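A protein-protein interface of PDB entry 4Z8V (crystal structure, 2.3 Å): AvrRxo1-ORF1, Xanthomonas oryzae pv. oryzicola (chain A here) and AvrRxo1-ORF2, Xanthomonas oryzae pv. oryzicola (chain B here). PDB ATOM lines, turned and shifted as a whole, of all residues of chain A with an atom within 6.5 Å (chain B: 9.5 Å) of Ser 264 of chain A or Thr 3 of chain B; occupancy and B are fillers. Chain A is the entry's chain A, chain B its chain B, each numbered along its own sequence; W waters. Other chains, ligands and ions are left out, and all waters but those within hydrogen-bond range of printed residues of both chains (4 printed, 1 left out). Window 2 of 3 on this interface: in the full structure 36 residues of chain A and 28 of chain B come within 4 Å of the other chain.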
ATOM      1  N   VAL A 255       6.026  -3.229   6.660  1.00  0.00           N
ATOM      2  CA  VAL A 255       5.572  -3.739   5.381  1.00  0.00           C
ATOM      3  C   VAL A 255       4.169  -3.214   5.048  1.00  0.00           C
ATOM      4  O   VAL A 255       3.913  -2.776   3.929  1.00  0.00           O
ATOM      5  CB  VAL A 255       5.573  -5.271   5.407  1.00  0.00           C
ATOM      6  CG1 VAL A 255       4.908  -5.832   4.165  1.00  0.00           C
ATOM      7  CG2 VAL A 255       7.009  -5.796   5.563  1.00  0.00           C
ATOM      8  N   ALA A 256       3.269  -3.246   6.024  1.00  0.00           N
ATOM      9  CA  ALA A 256       1.912  -2.746   5.832  1.00  0.00           C
ATOM     10  C   ALA A 256       1.404  -2.195   7.144  1.00  0.00           C
ATOM     11  O   ALA A 256       1.862  -2.598   8.217  1.00  0.00           O
ATOM     12  CB  ALA A 256       0.966  -3.866   5.332  1.00  0.00           C
ATOM     13  N   SER A 257       0.432  -1.292   7.081  1.00  0.00           N
ATOM     14  CA  SER A 257      -0.157  -0.808   8.315  1.00  0.00           C
ATOM     15  C   SER A 257      -1.561  -0.268   8.130  1.00  0.00           C
ATOM     16  O   SER A 257      -1.934   0.219   7.049  1.00  0.00           O
ATOM     17  CB  SER A 257       0.714   0.295   8.923  1.00  0.00           C
ATOM     18  OG  SER A 257       0.804   1.399   8.031  1.00  0.00           O
ATOM     19  N   VAL A 258      -2.335  -0.360   9.205  1.00  0.00           N
ATOM     20  CA  VAL A 258      -3.587   0.344   9.307  1.00  0.00           C
ATOM     21  C   VAL A 258      -3.515   1.191  10.575  1.00  0.00           C
ATOM     22  O   VAL A 258      -3.669   0.674  11.687  1.00  0.00           O
ATOM     23  CB  VAL A 258      -4.795  -0.596   9.368  1.00  0.00           C
ATOM     24  CG1 VAL A 258      -6.065   0.212   9.156  1.00  0.00           C
ATOM     25  CG2 VAL A 258      -4.686  -1.689   8.306  1.00  0.00           C
ATOM     26  N   ILE A 259      -3.267   2.486  10.400  1.00  0.00           N
ATOM     27  CA  ILE A 259      -3.149   3.390  11.533  1.00  0.00           C
ATOM     28  C   ILE A 259      -4.222   4.478  11.459  1.00  0.00           C
ATOM     29  O   ILE A 259      -4.171   5.334  10.573  1.00  0.00           O
ATOM     30  CB  ILE A 259      -1.748   4.038  11.582  1.00  0.00           C
ATOM     31  CG1 ILE A 259      -0.664   2.963  11.811  1.00  0.00           C
ATOM     32  CG2 ILE A 259      -1.713   5.106  12.676  1.00  0.00           C
ATOM     33  CD1 ILE A 259       0.722   3.345  11.292  1.00  0.00           C
ATOM     34  N   GLU A 262      -6.268   4.527   8.256  1.00  0.00           N
ATOM     35  CA  GLU A 262      -5.406   4.718   7.097  1.00  0.00           C
ATOM     36  C   GLU A 262      -4.646   3.418   6.785  1.00  0.00           C
ATOM     37  O   GLU A 262      -3.911   2.896   7.638  1.00  0.00           O
ATOM     38  CB  GLU A 262      -4.407   5.842   7.402  1.00  0.00           C
ATOM     39  CG  GLU A 262      -3.705   6.468   6.184  1.00  0.00           C
ATOM     40  CD  GLU A 262      -4.340   7.781   5.736  1.00  0.00           C
ATOM     41  OE1 GLU A 262      -5.122   8.381   6.522  1.00  0.00           O
ATOM     42  OE2 GLU A 262      -4.052   8.208   4.592  1.00  0.00           O
ATOM     43  N   PHE A 263      -4.820   2.905   5.571  1.00  0.00           N
ATOM     44  CA  PHE A 263      -4.136   1.700   5.118  1.00  0.00           C
ATOM     45  C   PHE A 263      -3.083   2.020   4.072  1.00  0.00           C
ATOM     46  O   PHE A 263      -3.380   2.656   3.048  1.00  0.00           O
ATOM     47  CB  PHE A 263      -5.115   0.700   4.509  1.00  0.00           C
ATOM     48  CG  PHE A 263      -4.444  -0.522   3.920  1.00  0.00           C
ATOM     49  CD1 PHE A 263      -3.713  -1.399   4.730  1.00  0.00           C
ATOM     50  CD2 PHE A 263      -4.559  -0.806   2.570  1.00  0.00           C
ATOM     51  CE1 PHE A 263      -3.107  -2.529   4.198  1.00  0.00           C
ATOM     52  CE2 PHE A 263      -3.961  -1.944   2.024  1.00  0.00           C
ATOM     53  CZ  PHE A 263      -3.231  -2.805   2.836  1.00  0.00           C
ATOM     54  N   SER A 264      -1.864   1.558   4.331  1.00  0.00           N
ATOM     55  CA  SER A 264      -0.742   1.806   3.448  1.00  0.00           C
ATOM     56  C   SER A 264       0.098   0.555   3.344  1.00  0.00           C
ATOM     57  O   SER A 264       0.111  -0.276   4.260  1.00  0.00           O
ATOM     58  CB  SER A 264       0.116   2.945   4.003  1.00  0.00           C
ATOM     59  OG  SER A 264      -0.697   4.072   4.270  1.00  0.00           O
ATOM     60  N   VAL A 265       0.802   0.425   2.227  1.00  0.00           N
ATOM     61  CA  VAL A 265       1.744  -0.668   2.045  1.00  0.00           C
ATOM     62  C   VAL A 265       3.158  -0.120   1.866  1.00  0.00           C
ATOM     63  O   VAL A 265       3.552   0.299   0.759  1.00  0.00           O
ATOM     64  CB  VAL A 265       1.376  -1.538   0.824  1.00  0.00           C
ATOM     65  CG1 VAL A 265       2.371  -2.695   0.689  1.00  0.00           C
ATOM     66  CG2 VAL A 265      -0.053  -2.080   0.964  1.00  0.00           C
ATOM     67  N   GLU A 266       3.928  -0.132   2.949  1.00  0.00           N
ATOM     68  CA  GLU A 266       5.277   0.434   2.916  1.00  0.00           C
ATOM     69  C   GLU A 266       6.253  -0.399   2.087  1.00  0.00           C
ATOM     70  O   GLU A 266       7.285   0.114   1.637  1.00  0.00           O
ATOM     71  CB  GLU A 266       5.803   0.670   4.338  1.00  0.00           C
ATOM     72  CG  GLU A 266       5.024   1.743   5.117  1.00  0.00           C
ATOM     73  CD  GLU A 266       3.760   1.192   5.743  1.00  0.00           C
ATOM     74  OE1 GLU A 266       2.938   1.969   6.272  1.00  0.00           O
ATOM     75  OE2 GLU A 266       3.583  -0.041   5.727  1.00  0.00           O
ATOM     76  N   ASN A 267       5.920  -1.673   1.873  1.00  0.00           N
ATOM     77  CA  ASN A 267       6.780  -2.568   1.095  1.00  0.00           C
ATOM     78  C   ASN A 267       5.961  -3.644   0.396  1.00  0.00           C
ATOM     79  O   ASN A 267       5.774  -4.747   0.926  1.00  0.00           O
ATOM     80  CB  ASN A 267       7.875  -3.205   1.982  1.00  0.00           C
ATOM     81  CG  ASN A 267       9.046  -3.756   1.168  1.00  0.00           C
ATOM     82  OD1 ASN A 267       8.863  -4.323   0.092  1.00  0.00           O
ATOM     83  ND2 ASN A 267      10.258  -3.566   1.675  1.00  0.00           N
ATOM     84  N   MET B   1      11.353   1.011  -0.947  1.00  0.00           N
ATOM     85  CA  MET B   1      10.597   1.360  -2.145  1.00  0.00           C
ATOM     86  C   MET B   1       9.445   2.298  -1.781  1.00  0.00           C
ATOM     87  O   MET B   1       9.182   2.559  -0.591  1.00  0.00           O
ATOM     88  CB  MET B   1      10.076   0.094  -2.854  1.00  0.00           C
ATOM     89  CG  MET B   1       9.031  -0.712  -2.069  1.00  0.00           C
ATOM     90  SD  MET B   1       8.638  -2.336  -2.796  1.00  0.00           S
ATOM     91  CE  MET B   1       7.602  -1.888  -4.190  1.00  0.00           C
ATOM     92  N   LYS B   2       8.765   2.806  -2.802  1.00  0.00           N
ATOM     93  CA  LYS B   2       7.685   3.750  -2.580  1.00  0.00           C
ATOM     94  C   LYS B   2       6.523   3.096  -1.849  1.00  0.00           C
ATOM     95  O   LYS B   2       6.096   1.981  -2.170  1.00  0.00           O
ATOM     96  CB  LYS B   2       7.201   4.338  -3.905  1.00  0.00           C
ATOM     97  CG  LYS B   2       6.298   5.558  -3.731  1.00  0.00           C
ATOM     98  CD  LYS B   2       5.729   6.063  -5.058  1.00  0.00           C
ATOM     99  CE  LYS B   2       5.116   7.447  -4.881  1.00  0.00           C
ATOM    100  NZ  LYS B   2       4.268   7.522  -3.648  1.00  0.00           N
ATOM    101  N   THR B   3       6.028   3.799  -0.842  1.00  0.00           N
ATOM    102  CA  THR B   3       4.835   3.378  -0.117  1.00  0.00           C
ATOM    103  C   THR B   3       3.601   3.545  -1.007  1.00  0.00           C
ATOM    104  O   THR B   3       3.420   4.582  -1.655  1.00  0.00           O
ATOM    105  CB  THR B   3       4.682   4.178   1.189  1.00  0.00           C
ATOM    106  OG1 THR B   3       5.821   3.920   2.026  1.00  0.00           O
ATOM    107  CG2 THR B   3       3.395   3.798   1.925  1.00  0.00           C
ATOM    108  N   LEU B   4       2.773   2.505  -1.056  1.00  0.00           N
ATOM    109  CA  LEU B   4       1.482   2.556  -1.750  1.00  0.00           C
ATOM    110  C   LEU B   4       0.462   3.137  -0.771  1.00  0.00           C
ATOM    111  O   LEU B   4       0.414   2.731   0.399  1.00  0.00           O
ATOM    112  CB  LEU B   4       1.041   1.149  -2.158  1.00  0.00           C
ATOM    113  CG  LEU B   4       1.457   0.518  -3.491  1.00  0.00           C
ATOM    114  CD1 LEU B   4       2.841   0.934  -3.957  1.00  0.00           C
ATOM    115  CD2 LEU B   4       1.350  -1.014  -3.400  1.00  0.00           C
ATOM    116  N   THR B   5      -0.349   4.082  -1.237  1.00  0.00           N
ATOM    117  CA  THR B   5      -1.301   4.771  -0.371  1.00  0.00           C
ATOM    118  C   THR B   5      -2.692   4.759  -1.001  1.00  0.00           C
ATOM    119  O   THR B   5      -2.845   4.336  -2.154  1.00  0.00           O
ATOM    120  CB  THR B   5      -0.840   6.228  -0.102  1.00  0.00           C
ATOM    121  OG1 THR B   5      -0.810   6.960  -1.331  1.00  0.00           O
ATOM    122  CG2 THR B   5       0.568   6.249   0.486  1.00  0.00           C
ATOM    123  N   GLY B   6      -3.694   5.197  -0.244  1.00  0.00           N
ATOM    124  CA  GLY B   6      -5.043   5.391  -0.752  1.00  0.00           C
ATOM    125  C   GLY B   6      -5.571   4.245  -1.585  1.00  0.00           C
ATOM    126  O   GLY B   6      -5.582   3.092  -1.149  1.00  0.00           O
ATOM    127  N   ALA B   7      -6.005   4.560  -2.799  1.00  0.00           N
ATOM    128  CA  ALA B   7      -6.680   3.588  -3.653  1.00  0.00           C
ATOM    129  C   ALA B   7      -5.728   2.510  -4.171  1.00  0.00           C
ATOM    130  O   ALA B   7      -6.135   1.361  -4.361  1.00  0.00           O
ATOM    131  CB  ALA B   7      -7.367   4.302  -4.817  1.00  0.00           C
ATOM    132  N   ASP B   8      -4.473   2.878  -4.420  1.00  0.00           N
ATOM    133  CA  ASP B   8      -3.482   1.904  -4.881  1.00  0.00           C
ATOM    134  C   ASP B   8      -3.194   0.846  -3.824  1.00  0.00           C
ATOM    135  O   ASP B   8      -3.141  -0.344  -4.134  1.00  0.00           O
ATOM    136  CB  ASP B   8      -2.183   2.595  -5.299  1.00  0.00           C
ATOM    137  CG  ASP B   8      -2.265   3.210  -6.684  1.00  0.00           C
ATOM    138  OD1 ASP B   8      -3.175   2.825  -7.455  1.00  0.00           O
ATOM    139  OD2 ASP B   8      -1.406   4.071  -6.998  1.00  0.00           O
ATOM    140  N   ALA B   9      -3.012   1.273  -2.575  1.00  0.00           N
ATOM    141  CA  ALA B   9      -2.804   0.327  -1.480  1.00  0.00           C
ATOM    142  C   ALA B   9      -3.975  -0.636  -1.389  1.00  0.00           C
ATOM    143  O   ALA B   9      -3.774  -1.854  -1.271  1.00  0.00           O
ATOM    144  CB  ALA B   9      -2.613   1.049  -0.151  1.00  0.00           C
ATOM    145  N   LEU B  10      -5.195  -0.093  -1.429  1.00  0.00           N
ATOM    146  CA  LEU B  10      -6.402  -0.920  -1.331  1.00  0.00           C
ATOM    147  C   LEU B  10      -6.486  -1.917  -2.473  1.00  0.00           C
ATOM    148  O   LEU B  10      -6.856  -3.071  -2.271  1.00  0.00           O
ATOM    149  CB  LEU B  10      -7.662  -0.060  -1.353  1.00  0.00           C
ATOM    150  CG  LEU B  10      -8.032   0.710  -0.092  1.00  0.00           C
ATOM    151  CD1 LEU B  10      -9.357   1.457  -0.301  1.00  0.00           C
ATOM    152  CD2 LEU B  10      -8.127  -0.230   1.103  1.00  0.00           C
ATOM    153  N   PHE B  12      -3.990  -3.023  -4.415  1.00  0.00           N
ATOM    154  CA  PHE B  12      -2.919  -4.002  -4.311  1.00  0.00           C
ATOM    155  C   PHE B  12      -3.346  -5.046  -3.295  1.00  0.00           C
ATOM    156  O   PHE B  12      -3.159  -6.237  -3.485  1.00  0.00           O
ATOM    157  CB  PHE B  12      -1.630  -3.325  -3.852  1.00  0.00           C
ATOM    158  CG  PHE B  12      -0.405  -4.187  -4.006  1.00  0.00           C
ATOM    159  CD1 PHE B  12       0.334  -4.164  -5.188  1.00  0.00           C
ATOM    160  CD2 PHE B  12       0.012  -5.017  -2.982  1.00  0.00           C
ATOM    161  CE1 PHE B  12       1.453  -4.959  -5.349  1.00  0.00           C
ATOM    162  CE2 PHE B  12       1.141  -5.811  -3.131  1.00  0.00           C
ATOM    163  CZ  PHE B  12       1.863  -5.780  -4.320  1.00  0.00           C
ATOM    164  N   HIS B  13      -3.950  -4.586  -2.213  1.00  0.00           N
ATOM    165  CA  HIS B  13      -4.419  -5.487  -1.174  1.00  0.00           C
ATOM    166  C   HIS B  13      -5.514  -6.449  -1.688  1.00  0.00           C
ATOM    167  O   HIS B  13      -5.482  -7.664  -1.415  1.00  0.00           O
ATOM    168  CB  HIS B  13      -4.929  -4.652   0.003  1.00  0.00           C
ATOM    169  CG  HIS B  13      -5.503  -5.460   1.117  1.00  0.00           C
ATOM    170  ND1 HIS B  13      -4.717  -6.105   2.054  1.00  0.00           N
ATOM    171  CD2 HIS B  13      -6.790  -5.724   1.457  1.00  0.00           C
ATOM    172  CE1 HIS B  13      -5.500  -6.722   2.925  1.00  0.00           C
ATOM    173  NE2 HIS B  13      -6.758  -6.512   2.583  1.00  0.00           N
HETATM  174  O   HOH W   1      -5.683   2.802   1.589  1.00  0.00           O
HETATM  175  O   HOH W   2      -2.556   5.354   2.789  1.00  0.00           O
HETATM  176  O   HOH W   3       5.284  -0.281  -1.386  1.00  0.00           O
HETATM  177  O   HOH W   4      10.031  -0.408   1.101  1.00  0.00           O
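Of the 12 printed residues of chain B, 6 touch a printed residue of chain A. Hydrophobic or aromatic side chains of chain B that line the printed part of chain A: Met 1, Leu 4, Ala 9, Leu 10 and His 13. Hydrophobic or aromatic side chains of chain A within 4 Å of the printed part of chain B: Phe 263. Along chain A the printed residues that touch a printed residue of chain B span positions 263 to 267. Among the printed residues, 10 pairs touch across the chains. Among the printed residues, no Asp or Glu carboxylate lies within 4 Å of a Lys or Arg side-chain nitrogen of the other chain.
Ser 264 of chain A touches two residues of chain B. No residue of chain B comes within 4 Å of Ser 257 of chain A. Val 265 of chain A touches two residues of chain B. Of chain B, only Met 1 (3.8 Å) and Thr 3 (3.6 Å) come within 4 Å of Glu 266 of chain A. Of the printed residues of chain A, Leu 10 of chain B touches Phe 263. Printed residues of chain A within 4 Å of Leu 4 of chain B: Ser 264 (3.4 Å) and Val 265 (3.0 Å). Of the printed residues of chain A, His 13 of chain B touches Phe 263. Printed residues of chain A within 4 Å of Ala 9 of chain B: Phe 263 (3.3 Å). Of the printed residues of chain A, Met 1 of chain B touches Glu 266 and Asn 267. The nearest residue of chain A that does not touch Thr 3 of chain B is Asn 267 of chain A (5.5 Å). The nearest printed residue of chain A that does not touch His 13 of chain B is Val 265 of chain A (5.6 Å).
Water W3 lies within hydrogen-bond range of O of Lys 2 of chain B (2.5 Å) and O of Val 265 of chain A (2.8 Å). Water W2 lies within hydrogen-bond range of OG of Ser 264 of chain A (2.7 Å), O of Phe 263 of chain A (2.8 Å) and N of Gly 6 of chain B (3.2 Å). Water W1 lies within hydrogen-bond range of the backbone carbonyl oxygen of Phe 263 of chain A and the backbone carbonyl oxygen of Gly 6 of chain B. Water W4 lies within hydrogen-bond range of N of Met 1 of chain B, O of Glu 266 of chain A and ND2 of Asn 267 of chain A.
The backbone carbonyl oxygen of Val 255 of chain A lies within hydrogen-bond range of the backbone NH of Glu 266 of chain A, 2.8 Å away. The backbone NH (N) of Asn 267 of chain A sits at hydrogen-bond distance from the backbone carbonyl oxygen (O) of Val 255 of chain A, 3.1 Å away. The backbone NH of Ala 256 of chain A sits close to the side-chain carboxylate of Glu 266 of chain A, at 3.2 Å. The backbone NH (N) of Ser 257 of chain A sits at hydrogen-bond distance from the backbone carbonyl oxygen (O) of Ser 264 of chain A. The side-chain carboxylate (OE1) of Glu 266 of chain A sits at hydrogen-bond distance from the side-chain hydroxyl (OG) of Ser 257 of chain A (2.8 Å).
Among the printed residues, pairs that only touch across the chains: Phe 263 of chain A with Ala 9 of chain B (3.3 Å), Phe 263 of chain A with Leu 10 of chain B (3.9 Å), Phe 263 of chain A with His 13 of chain B (3.5 Å), Ser 264 of chain A with Thr 3 of chain B (3.97 Å), Ser 264 of chain A with Leu 4 of chain B (3.4 Å), Val 265 of chain A with Thr 3 of chain B (3.4 Å), Glu 266 of chain A with Met 1 of chain B (3.8 Å) and Glu 266 of chain A with Thr 3 of chain B (3.6 Å).
N of Leu 4 of chain B sits at hydrogen-bond distance from O of Val 265 of chain A. The side-chain amide oxygen (OD1) of Asn 267 of chain A lies close to the side-chain sulfur (SD) of Met 1 of chain B.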
